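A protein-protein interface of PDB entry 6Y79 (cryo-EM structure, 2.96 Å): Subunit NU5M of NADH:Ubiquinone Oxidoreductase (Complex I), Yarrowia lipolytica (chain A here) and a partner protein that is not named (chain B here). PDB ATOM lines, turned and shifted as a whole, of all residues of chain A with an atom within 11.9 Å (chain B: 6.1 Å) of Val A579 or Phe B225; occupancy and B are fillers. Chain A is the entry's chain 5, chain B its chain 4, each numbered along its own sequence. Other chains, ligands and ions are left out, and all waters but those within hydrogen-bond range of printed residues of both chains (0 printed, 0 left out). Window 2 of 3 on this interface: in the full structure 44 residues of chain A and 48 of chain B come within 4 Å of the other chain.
A ring nitrogen (NE2) of His B228 lies within hydrogen-bond range of the side-chain carboxylate (OD2) of Asp A580.
O of Val A579 is in hydrogen-bond range of OG of Ser A583, at 3.3 Å.
The backbone carbonyl oxygen of Ile A575 lies within hydrogen-bond range of the backbone NH of Asp A580 (2.8 Å).
The backbone carbonyl oxygen (O) of Tyr A585 lies within hydrogen-bond range of the backbone NH (N) of Gly A591, at 3.0 Å.
The backbone carbonyl oxygen (O) of Tyr A585 sits at hydrogen-bond distance from the backbone NH (N) of Val A590 (3.0 Å).
The backbone carbonyl oxygen (O) of Asn A574 is in hydrogen-bond range of the backbone NH (N) of Val A579 (3.5 Å).
The backbone carbonyl oxygen (O) of Val A579 lies within hydrogen-bond range of the backbone NH (N) of Leu A584.
Ile A575 touches Leu B287 (CG2 to O, 3.9 Å).
Val A579 touches Phe B225.
Asp A580 touches Phe B225 (OD1 to CE1, 3.9 Å).
Phe B225 touches Leu A584 (CZ to CD1, 3.7 Å).
Leu A584 touches Pro B226 (CD2 to O, 3.9 Å).
Leu A584 touches His B228.
Tyr A585 touches Val B229.
Printed residues of chain B within 4 Å of Ile A575: Leu B287.
Val A579 touches just one residue of chain B: Phe B225 (3.97 Å).
Printed residues of chain B within 4 Å of Asp A580: Phe B225 and His B228.
Lys A581 touches none of the printed residues of chain B.
Gly A582 touches none of the printed residues of chain B.
Printed residues of chain B within 4 Å of Leu A584: Phe B225 (3.7 Å), Pro B226 (3.9 Å) and His B228 (3.5 Å).
No residue of chain A comes within 4 Å of Pro B223.
No residue of chain A comes within 4 Å of Leu B224.
Phe B225 touches just these residues of chain A: Val A579 (3.97 Å), Asp A580 (3.9 Å) and Leu A584 (3.7 Å).
Of chain A, only Leu A584 (3.9 Å) comes within 4 Å of Pro B226.
No residue of chain A comes within 4 Å of Ile B227.
His B228 touches just these residues of chain A: Asp A580 and Leu A584.
Printed residues of chain A within 4 Å of Val B229: Tyr A585 (3.5 Å).
No residue of chain A comes within 4 Å of Leu B283.
No residue of chain A comes within 4 Å of Thr B284.
Of the printed residues of chain A, Leu B287 touches Ile A575.
The nearest residue of chain A that does not touch Phe B225 is Ile A575 (5.6 Å).
The nearest printed residue of chain B that does not touch Ile A575 is Phe B225 (5.6 Å).
Of the 23 printed residues of chain A, 5 touch a printed residue of chain B.
Printed residues of chain B that touch a printed residue of chain A: Phe B225, Pro B226, His B228, Val B229 and Leu B287.
Hydrophobic or aromatic side chains of chain B within 4 Å of the printed part of chain A: Phe B225, His B228 and Val B229.
Among the printed residues, 8 pairs touch across the chains.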
ATOM      1  N   LEU A 569      28.962  -5.563  24.712  1.00  0.00           N
ATOM      2  CA  LEU A 569      30.210  -5.025  25.245  1.00  0.00           C
ATOM      3  C   LEU A 569      30.971  -4.228  24.193  1.00  0.00           C
ATOM      4  O   LEU A 569      31.600  -3.213  24.509  1.00  0.00           O
ATOM      5  CB  LEU A 569      31.082  -6.150  25.788  1.00  0.00           C
ATOM      6  CG  LEU A 569      30.634  -6.764  27.106  1.00  0.00           C
ATOM      7  CD1 LEU A 569      31.457  -7.989  27.408  1.00  0.00           C
ATOM      8  CD2 LEU A 569      30.774  -5.753  28.204  1.00  0.00           C
ATOM      9  N   VAL A 570      30.896  -4.645  22.930  1.00  0.00           N
ATOM     10  CA  VAL A 570      31.569  -3.896  21.873  1.00  0.00           C
ATOM     11  C   VAL A 570      30.860  -2.565  21.602  1.00  0.00           C
ATOM     12  O   VAL A 570      31.520  -1.531  21.447  1.00  0.00           O
ATOM     13  CB  VAL A 570      31.701  -4.774  20.618  1.00  0.00           C
ATOM     14  CG1 VAL A 570      32.093  -3.955  19.413  1.00  0.00           C
ATOM     15  CG2 VAL A 570      32.745  -5.833  20.859  1.00  0.00           C
ATOM     16  N   THR A 571      29.517  -2.547  21.601  1.00  0.00           N
ATOM     17  CA  THR A 571      28.825  -1.262  21.450  1.00  0.00           C
ATOM     18  C   THR A 571      29.008  -0.362  22.666  1.00  0.00           C
ATOM     19  O   THR A 571      29.058   0.864  22.521  1.00  0.00           O
ATOM     20  CB  THR A 571      27.325  -1.427  21.199  1.00  0.00           C
ATOM     21  OG1 THR A 571      26.678  -1.866  22.400  1.00  0.00           O
ATOM     22  CG2 THR A 571      27.025  -2.368  20.037  1.00  0.00           C
ATOM     23  N   SER A 572      29.124  -0.934  23.865  1.00  0.00           N
ATOM     24  CA  SER A 572      29.360  -0.112  25.045  1.00  0.00           C
ATOM     25  C   SER A 572      30.762   0.473  25.033  1.00  0.00           C
ATOM     26  O   SER A 572      30.970   1.595  25.500  1.00  0.00           O
ATOM     27  CB  SER A 572      29.133  -0.931  26.307  1.00  0.00           C
ATOM     28  OG  SER A 572      30.134  -1.903  26.483  1.00  0.00           O
ATOM     29  N   GLY A 573      31.734  -0.263  24.493  1.00  0.00           N
ATOM     30  CA  GLY A 573      33.045   0.320  24.279  1.00  0.00           C
ATOM     31  C   GLY A 573      33.050   1.381  23.201  1.00  0.00           C
ATOM     32  O   GLY A 573      33.796   2.360  23.299  1.00  0.00           O
ATOM     33  N   ASN A 574      32.216   1.205  22.170  1.00  0.00           N
ATOM     34  CA  ASN A 574      32.020   2.242  21.162  1.00  0.00           C
ATOM     35  C   ASN A 574      31.497   3.526  21.783  1.00  0.00           C
ATOM     36  O   ASN A 574      31.938   4.616  21.415  1.00  0.00           O
ATOM     37  CB  ASN A 574      31.051   1.766  20.082  1.00  0.00           C
ATOM     38  CG  ASN A 574      31.676   0.792  19.127  1.00  0.00           C
ATOM     39  OD1 ASN A 574      32.876   0.839  18.878  1.00  0.00           O
ATOM     40  ND2 ASN A 574      30.864  -0.097  18.575  1.00  0.00           N
ATOM     41  N   ILE A 575      30.563   3.419  22.725  1.00  0.00           N
ATOM     42  CA  ILE A 575      30.027   4.611  23.378  1.00  0.00           C
ATOM     43  C   ILE A 575      31.050   5.213  24.334  1.00  0.00           C
ATOM     44  O   ILE A 575      31.290   6.424  24.324  1.00  0.00           O
ATOM     45  CB  ILE A 575      28.706   4.286  24.088  1.00  0.00           C
ATOM     46  CG1 ILE A 575      27.657   3.927  23.046  1.00  0.00           C
ATOM     47  CG2 ILE A 575      28.250   5.448  24.931  1.00  0.00           C
ATOM     48  CD1 ILE A 575      26.307   3.760  23.607  1.00  0.00           C
ATOM     49  N   ALA A 576      31.698   4.374  25.141  1.00  0.00           N
ATOM     50  CA  ALA A 576      32.635   4.859  26.142  1.00  0.00           C
ATOM     51  C   ALA A 576      33.899   5.449  25.538  1.00  0.00           C
ATOM     52  O   ALA A 576      34.569   6.242  26.203  1.00  0.00           O
ATOM     53  CB  ALA A 576      32.997   3.728  27.097  1.00  0.00           C
ATOM     54  N   HIS A 577      34.239   5.106  24.298  1.00  0.00           N
ATOM     55  CA  HIS A 577      35.414   5.679  23.662  1.00  0.00           C
ATOM     56  C   HIS A 577      35.079   6.677  22.566  1.00  0.00           C
ATOM     57  O   HIS A 577      35.612   7.785  22.563  1.00  0.00           O
ATOM     58  CB  HIS A 577      36.286   4.565  23.081  1.00  0.00           C
ATOM     59  CG  HIS A 577      36.846   3.639  24.108  1.00  0.00           C
ATOM     60  ND1 HIS A 577      36.170   2.522  24.548  1.00  0.00           N
ATOM     61  CD2 HIS A 577      38.019   3.657  24.779  1.00  0.00           C
ATOM     62  CE1 HIS A 577      36.901   1.893  25.448  1.00  0.00           C
ATOM     63  NE2 HIS A 577      38.029   2.561  25.606  1.00  0.00           N
ATOM     64  N   HIS A 578      34.222   6.310  21.619  1.00  0.00           N
ATOM     65  CA  HIS A 578      33.990   7.133  20.445  1.00  0.00           C
ATOM     66  C   HIS A 578      32.973   8.234  20.677  1.00  0.00           C
ATOM     67  O   HIS A 578      32.980   9.224  19.943  1.00  0.00           O
ATOM     68  CB  HIS A 578      33.530   6.263  19.276  1.00  0.00           C
ATOM     69  CG  HIS A 578      34.514   5.205  18.901  1.00  0.00           C
ATOM     70  ND1 HIS A 578      35.749   5.499  18.372  1.00  0.00           N
ATOM     71  CD2 HIS A 578      34.451   3.858  18.985  1.00  0.00           C
ATOM     72  CE1 HIS A 578      36.407   4.377  18.147  1.00  0.00           C
ATOM     73  NE2 HIS A 578      35.641   3.366  18.512  1.00  0.00           N
ATOM     74  N   VAL A 579      32.098   8.091  21.661  1.00  0.00           N
ATOM     75  CA  VAL A 579      31.062   9.078  21.939  1.00  0.00           C
ATOM     76  C   VAL A 579      31.392   9.888  23.183  1.00  0.00           C
ATOM     77  O   VAL A 579      31.459  11.114  23.134  1.00  0.00           O
ATOM     78  CB  VAL A 579      29.673   8.411  22.053  1.00  0.00           C
ATOM     79  CG1 VAL A 579      28.633   9.427  22.454  1.00  0.00           C
ATOM     80  CG2 VAL A 579      29.298   7.773  20.748  1.00  0.00           C
ATOM     81  N   ASP A 580      31.627   9.218  24.310  1.00  0.00           N
ATOM     82  CA  ASP A 580      31.766   9.929  25.575  1.00  0.00           C
ATOM     83  C   ASP A 580      33.158  10.514  25.738  1.00  0.00           C
ATOM     84  O   ASP A 580      33.301  11.681  26.089  1.00  0.00           O
ATOM     85  CB  ASP A 580      31.417   9.015  26.743  1.00  0.00           C
ATOM     86  CG  ASP A 580      29.930   8.743  26.832  1.00  0.00           C
ATOM     87  OD1 ASP A 580      29.235   8.892  25.802  1.00  0.00           O
ATOM     88  OD2 ASP A 580      29.448   8.392  27.930  1.00  0.00           O
ATOM     89  N   LYS A 581      34.197   9.725  25.499  1.00  0.00           N
ATOM     90  CA  LYS A 581      35.543  10.278  25.500  1.00  0.00           C
ATOM     91  C   LYS A 581      35.969  10.794  24.141  1.00  0.00           C
ATOM     92  O   LYS A 581      36.998  11.462  24.045  1.00  0.00           O
ATOM     93  CB  LYS A 581      36.553   9.243  25.984  1.00  0.00           C
ATOM     94  CG  LYS A 581      36.560   9.094  27.478  1.00  0.00           C
ATOM     95  CD  LYS A 581      37.589   8.105  27.942  1.00  0.00           C
ATOM     96  CE  LYS A 581      37.444   7.858  29.428  1.00  0.00           C
ATOM     97  NZ  LYS A 581      38.353   6.792  29.913  1.00  0.00           N
ATOM     98  N   GLY A 582      35.239  10.467  23.090  1.00  0.00           N
ATOM     99  CA  GLY A 582      35.613  10.961  21.792  1.00  0.00           C
ATOM    100  C   GLY A 582      34.997  12.248  21.301  1.00  0.00           C
ATOM    101  O   GLY A 582      35.704  13.227  21.065  1.00  0.00           O
ATOM    102  N   SER A 583      33.681  12.274  21.146  1.00  0.00           N
ATOM    103  CA  SER A 583      33.047  13.383  20.457  1.00  0.00           C
ATOM    104  C   SER A 583      32.340  14.342  21.395  1.00  0.00           C
ATOM    105  O   SER A 583      32.038  15.466  20.992  1.00  0.00           O
ATOM    106  CB  SER A 583      32.053  12.870  19.416  1.00  0.00           C
ATOM    107  OG  SER A 583      30.992  12.184  20.040  1.00  0.00           O
ATOM    108  N   LEU A 584      32.061  13.925  22.624  1.00  0.00           N
ATOM    109  CA  LEU A 584      31.576  14.853  23.630  1.00  0.00           C
ATOM    110  C   LEU A 584      32.705  15.625  24.293  1.00  0.00           C
ATOM    111  O   LEU A 584      32.434  16.524  25.091  1.00  0.00           O
ATOM    112  CB  LEU A 584      30.771  14.116  24.690  1.00  0.00           C
ATOM    113  CG  LEU A 584      29.448  13.563  24.176  1.00  0.00           C
ATOM    114  CD1 LEU A 584      28.803  12.694  25.213  1.00  0.00           C
ATOM    115  CD2 LEU A 584      28.530  14.683  23.779  1.00  0.00           C
ATOM    116  N   TYR A 585      33.963  15.295  23.993  1.00  0.00           N
ATOM    117  CA  TYR A 585      35.081  16.134  24.403  1.00  0.00           C
ATOM    118  C   TYR A 585      35.543  17.038  23.286  1.00  0.00           C
ATOM    119  O   TYR A 585      36.271  17.997  23.540  1.00  0.00           O
ATOM    120  CB  TYR A 585      36.307  15.345  24.840  1.00  0.00           C
ATOM    121  CG  TYR A 585      36.246  14.570  26.122  1.00  0.00           C
ATOM    122  CD1 TYR A 585      35.064  14.153  26.710  1.00  0.00           C
ATOM    123  CD2 TYR A 585      37.429  14.316  26.811  1.00  0.00           C
ATOM    124  CE1 TYR A 585      35.103  13.452  27.878  1.00  0.00           C
ATOM    125  CE2 TYR A 585      37.443  13.617  27.970  1.00  0.00           C
ATOM    126  CZ  TYR A 585      36.240  13.198  28.491  1.00  0.00           C
ATOM    127  OH  TYR A 585      36.234  12.476  29.687  1.00  0.00           O
ATOM    128  N   ARG A 586      35.205  16.706  22.046  1.00  0.00           N
ATOM    129  CA  ARG A 586      35.522  17.595  20.944  1.00  0.00           C
ATOM    130  C   ARG A 586      34.599  18.798  20.954  1.00  0.00           C
ATOM    131  O   ARG A 586      35.007  19.900  20.576  1.00  0.00           O
ATOM    132  CB  ARG A 586      35.435  16.829  19.628  1.00  0.00           C
ATOM    133  CG  ARG A 586      36.158  17.490  18.495  1.00  0.00           C
ATOM    134  CD  ARG A 586      37.598  17.783  18.845  1.00  0.00           C
ATOM    135  NE  ARG A 586      38.353  16.569  19.106  1.00  0.00           N
ATOM    136  CZ  ARG A 586      38.982  15.877  18.166  1.00  0.00           C
ATOM    137  NH1 ARG A 586      38.939  16.282  16.908  1.00  0.00           N
ATOM    138  NH2 ARG A 586      39.653  14.783  18.480  1.00  0.00           N
ATOM    139  N   LEU A 587      33.363  18.607  21.400  1.00  0.00           N
ATOM    140  CA  LEU A 587      32.469  19.699  21.742  1.00  0.00           C
ATOM    141  C   LEU A 587      32.679  20.200  23.160  1.00  0.00           C
ATOM    142  O   LEU A 587      32.000  21.137  23.577  1.00  0.00           O
ATOM    143  CB  LEU A 587      31.017  19.261  21.567  1.00  0.00           C
ATOM    144  CG  LEU A 587      30.589  19.065  20.117  1.00  0.00           C
ATOM    145  CD1 LEU A 587      29.171  18.541  20.041  1.00  0.00           C
ATOM    146  CD2 LEU A 587      30.728  20.365  19.352  1.00  0.00           C
ATOM    147  N   GLY A 588      33.591  19.596  23.905  1.00  0.00           N
ATOM    148  CA  GLY A 588      33.843  19.977  25.267  1.00  0.00           C
ATOM    149  C   GLY A 588      35.260  20.460  25.448  1.00  0.00           C
ATOM    150  O   GLY A 588      35.784  21.219  24.635  1.00  0.00           O
ATOM    151  N   PRO A 589      35.926  19.992  26.503  1.00  0.00           N
ATOM    152  CA  PRO A 589      37.179  20.630  26.926  1.00  0.00           C
ATOM    153  C   PRO A 589      38.392  20.335  26.058  1.00  0.00           C
ATOM    154  O   PRO A 589      39.403  21.027  26.209  1.00  0.00           O
ATOM    155  CB  PRO A 589      37.379  20.086  28.342  1.00  0.00           C
ATOM    156  CG  PRO A 589      36.611  18.839  28.388  1.00  0.00           C
ATOM    157  CD  PRO A 589      35.447  19.006  27.483  1.00  0.00           C
ATOM    158  N   VAL A 590      38.333  19.361  25.159  1.00  0.00           N
ATOM    159  CA  VAL A 590      39.498  18.951  24.380  1.00  0.00           C
ATOM    160  C   VAL A 590      39.503  19.680  23.042  1.00  0.00           C
ATOM    161  O   VAL A 590      40.565  20.019  22.509  1.00  0.00           O
ATOM    162  CB  VAL A 590      39.517  17.418  24.223  1.00  0.00           C
ATOM    163  CG1 VAL A 590      40.705  16.939  23.427  1.00  0.00           C
ATOM    164  CG2 VAL A 590      39.611  16.807  25.577  1.00  0.00           C
ATOM    165  N   GLY A 591      38.322  19.987  22.518  1.00  0.00           N
ATOM    166  CA  GLY A 591      38.235  20.712  21.269  1.00  0.00           C
ATOM    167  C   GLY A 591      38.302  22.211  21.455  1.00  0.00           C
ATOM    168  O   GLY A 591      38.839  22.937  20.610  1.00  0.00           O
ATOM    169  N   MET B 219      20.798  20.800  33.474  1.00  0.00           N
ATOM    170  CA  MET B 219      21.414  19.763  32.660  1.00  0.00           C
ATOM    171  C   MET B 219      22.909  19.663  32.928  1.00  0.00           C
ATOM    172  O   MET B 219      23.485  18.574  32.869  1.00  0.00           O
ATOM    173  CB  MET B 219      21.137  20.048  31.187  1.00  0.00           C
ATOM    174  CG  MET B 219      21.815  19.117  30.218  1.00  0.00           C
ATOM    175  SD  MET B 219      21.601  19.621  28.525  1.00  0.00           S
ATOM    176  CE  MET B 219      19.831  19.602  28.478  1.00  0.00           C
ATOM    177  N   PRO B 223      23.798  15.982  35.864  1.00  0.00           N
ATOM    178  CA  PRO B 223      24.415  15.929  34.547  1.00  0.00           C
ATOM    179  C   PRO B 223      23.692  14.989  33.606  1.00  0.00           C
ATOM    180  O   PRO B 223      23.794  13.762  33.693  1.00  0.00           O
ATOM    181  CB  PRO B 223      25.838  15.470  34.870  1.00  0.00           C
ATOM    182  CG  PRO B 223      26.023  15.807  36.262  1.00  0.00           C
ATOM    183  CD  PRO B 223      24.723  15.451  36.867  1.00  0.00           C
ATOM    184  N   LEU B 224      22.922  15.596  32.720  1.00  0.00           N
ATOM    185  CA  LEU B 224      22.223  14.893  31.667  1.00  0.00           C
ATOM    186  C   LEU B 224      23.122  14.837  30.444  1.00  0.00           C
ATOM    187  O   LEU B 224      24.114  15.559  30.367  1.00  0.00           O
ATOM    188  CB  LEU B 224      20.904  15.592  31.371  1.00  0.00           C
ATOM    189  CG  LEU B 224      20.005  15.817  32.588  1.00  0.00           C
ATOM    190  CD1 LEU B 224      18.847  16.726  32.258  1.00  0.00           C
ATOM    191  CD2 LEU B 224      19.501  14.507  33.131  1.00  0.00           C
ATOM    192  N   PHE B 225      22.741  13.995  29.480  1.00  0.00           N
ATOM    193  CA  PHE B 225      23.680  13.447  28.495  1.00  0.00           C
ATOM    194  C   PHE B 225      24.538  14.428  27.684  1.00  0.00           C
ATOM    195  O   PHE B 225      25.704  14.079  27.431  1.00  0.00           O
ATOM    196  CB  PHE B 225      22.950  12.523  27.504  1.00  0.00           C
ATOM    197  CG  PHE B 225      23.880  11.874  26.508  1.00  0.00           C
ATOM    198  CD1 PHE B 225      24.708  10.842  26.904  1.00  0.00           C
ATOM    199  CD2 PHE B 225      23.978  12.342  25.202  1.00  0.00           C
ATOM    200  CE1 PHE B 225      25.582  10.266  26.015  1.00  0.00           C
ATOM    201  CE2 PHE B 225      24.837  11.771  24.319  1.00  0.00           C
ATOM    202  CZ  PHE B 225      25.649  10.735  24.721  1.00  0.00           C
ATOM    203  N   PRO B 226      24.058  15.594  27.199  1.00  0.00           N
ATOM    204  CA  PRO B 226      24.975  16.459  26.430  1.00  0.00           C
ATOM    205  C   PRO B 226      26.194  16.930  27.212  1.00  0.00           C
ATOM    206  O   PRO B 226      27.295  16.966  26.656  1.00  0.00           O
ATOM    207  CB  PRO B 226      24.079  17.633  26.023  1.00  0.00           C
ATOM    208  CG  PRO B 226      22.753  17.061  25.952  1.00  0.00           C
ATOM    209  CD  PRO B 226      22.677  16.112  27.091  1.00  0.00           C
ATOM    210  N   ILE B 227      26.041  17.243  28.497  1.00  0.00           N
ATOM    211  CA  ILE B 227      27.168  17.553  29.374  1.00  0.00           C
ATOM    212  C   ILE B 227      26.975  16.730  30.649  1.00  0.00           C
ATOM    213  O   ILE B 227      26.276  17.141  31.578  1.00  0.00           O
ATOM    214  CB  ILE B 227      27.290  19.051  29.683  1.00  0.00           C
ATOM    215  CG1 ILE B 227      27.613  19.865  28.425  1.00  0.00           C
ATOM    216  CG2 ILE B 227      28.414  19.308  30.635  1.00  0.00           C
ATOM    217  CD1 ILE B 227      26.423  20.475  27.716  1.00  0.00           C
ATOM    218  N   HIS B 228      27.573  15.542  30.691  1.00  0.00           N
ATOM    219  CA  HIS B 228      27.524  14.643  31.843  1.00  0.00           C
ATOM    220  C   HIS B 228      28.923  14.233  32.244  1.00  0.00           C
ATOM    221  O   HIS B 228      29.149  13.190  32.855  1.00  0.00           O
ATOM    222  CB  HIS B 228      26.683  13.403  31.560  1.00  0.00           C
ATOM    223  CG  HIS B 228      27.252  12.533  30.487  1.00  0.00           C
ATOM    224  ND1 HIS B 228      27.028  12.764  29.148  1.00  0.00           N
ATOM    225  CD2 HIS B 228      28.053  11.445  30.551  1.00  0.00           C
ATOM    226  CE1 HIS B 228      27.658  11.851  28.434  1.00  0.00           C
ATOM    227  NE2 HIS B 228      28.291  11.039  29.261  1.00  0.00           N
ATOM    228  N   VAL B 229      29.859  15.126  31.970  1.00  0.00           N
ATOM    229  CA  VAL B 229      31.165  14.754  31.460  1.00  0.00           C
ATOM    230  C   VAL B 229      32.289  15.230  32.376  1.00  0.00           C
ATOM    231  O   VAL B 229      33.320  14.567  32.515  1.00  0.00           O
ATOM    232  CB  VAL B 229      31.266  15.316  30.019  1.00  0.00           C
ATOM    233  CG1 VAL B 229      32.666  15.395  29.497  1.00  0.00           C
ATOM    234  CG2 VAL B 229      30.441  14.442  29.100  1.00  0.00           C
ATOM    235  N   ILE B 280      16.061  13.504  26.857  1.00  0.00           N
ATOM    236  CA  ILE B 280      17.374  13.708  27.459  1.00  0.00           C
ATOM    237  C   ILE B 280      17.593  12.794  28.664  1.00  0.00           C
ATOM    238  O   ILE B 280      18.695  12.274  28.863  1.00  0.00           O
ATOM    239  CB  ILE B 280      17.534  15.197  27.806  1.00  0.00           C
ATOM    240  CG1 ILE B 280      17.483  16.019  26.532  1.00  0.00           C
ATOM    241  CG2 ILE B 280      18.856  15.477  28.392  1.00  0.00           C
ATOM    242  CD1 ILE B 280      17.276  17.471  26.778  1.00  0.00           C
ATOM    243  N   LEU B 283      17.890   9.150  27.520  1.00  0.00           N
ATOM    244  CA  LEU B 283      19.114   9.070  26.762  1.00  0.00           C
ATOM    245  C   LEU B 283      20.346   9.231  27.632  1.00  0.00           C
ATOM    246  O   LEU B 283      21.438   8.867  27.201  1.00  0.00           O
ATOM    247  CB  LEU B 283      19.015  10.136  25.682  1.00  0.00           C
ATOM    248  CG  LEU B 283      19.876  10.313  24.469  1.00  0.00           C
ATOM    249  CD1 LEU B 283      18.913  10.589  23.385  1.00  0.00           C
ATOM    250  CD2 LEU B 283      20.629  11.543  24.724  1.00  0.00           C
ATOM    251  N   THR B 284      20.200   9.768  28.842  1.00  0.00           N
ATOM    252  CA  THR B 284      21.282   9.757  29.817  1.00  0.00           C
ATOM    253  C   THR B 284      21.186   8.601  30.800  1.00  0.00           C
ATOM    254  O   THR B 284      22.158   8.335  31.507  1.00  0.00           O
ATOM    255  CB  THR B 284      21.338  11.080  30.596  1.00  0.00           C
ATOM    256  OG1 THR B 284      22.605  11.191  31.247  1.00  0.00           O
ATOM    257  CG2 THR B 284      20.285  11.141  31.653  1.00  0.00           C
ATOM    258  N   LEU B 287      22.588   5.542  27.839  1.00  0.00           N
ATOM    259  CA  LEU B 287      23.916   5.672  27.262  1.00  0.00           C
ATOM    260  C   LEU B 287      24.997   5.775  28.321  1.00  0.00           C
ATOM    261  O   LEU B 287      26.095   5.247  28.123  1.00  0.00           O
ATOM    262  CB  LEU B 287      23.956   6.876  26.318  1.00  0.00           C
ATOM    263  CG  LEU B 287      23.556   6.578  24.866  1.00  0.00           C
ATOM    264  CD1 LEU B 287      22.076   6.280  24.672  1.00  0.00           C
ATOM    265  CD2 LEU B 287      23.943   7.713  23.973  1.00  0.00           C
ATOM    266  N   THR B 288      24.701   6.384  29.460  1.00  0.00           N
ATOM    267  CA  THR B 288      25.657   6.371  30.554  1.00  0.00           C
ATOM    268  C   THR B 288      25.721   5.020  31.251  1.00  0.00           C
ATOM    269  O   THR B 288      26.825   4.533  31.521  1.00  0.00           O
ATOM    270  CB  THR B 288      25.324   7.460  31.565  1.00  0.00           C
ATOM    271  OG1 THR B 288      25.338   8.731  30.911  1.00  0.00           O
ATOM    272  CG2 THR B 288      26.349   7.478  32.619  1.00  0.00           C
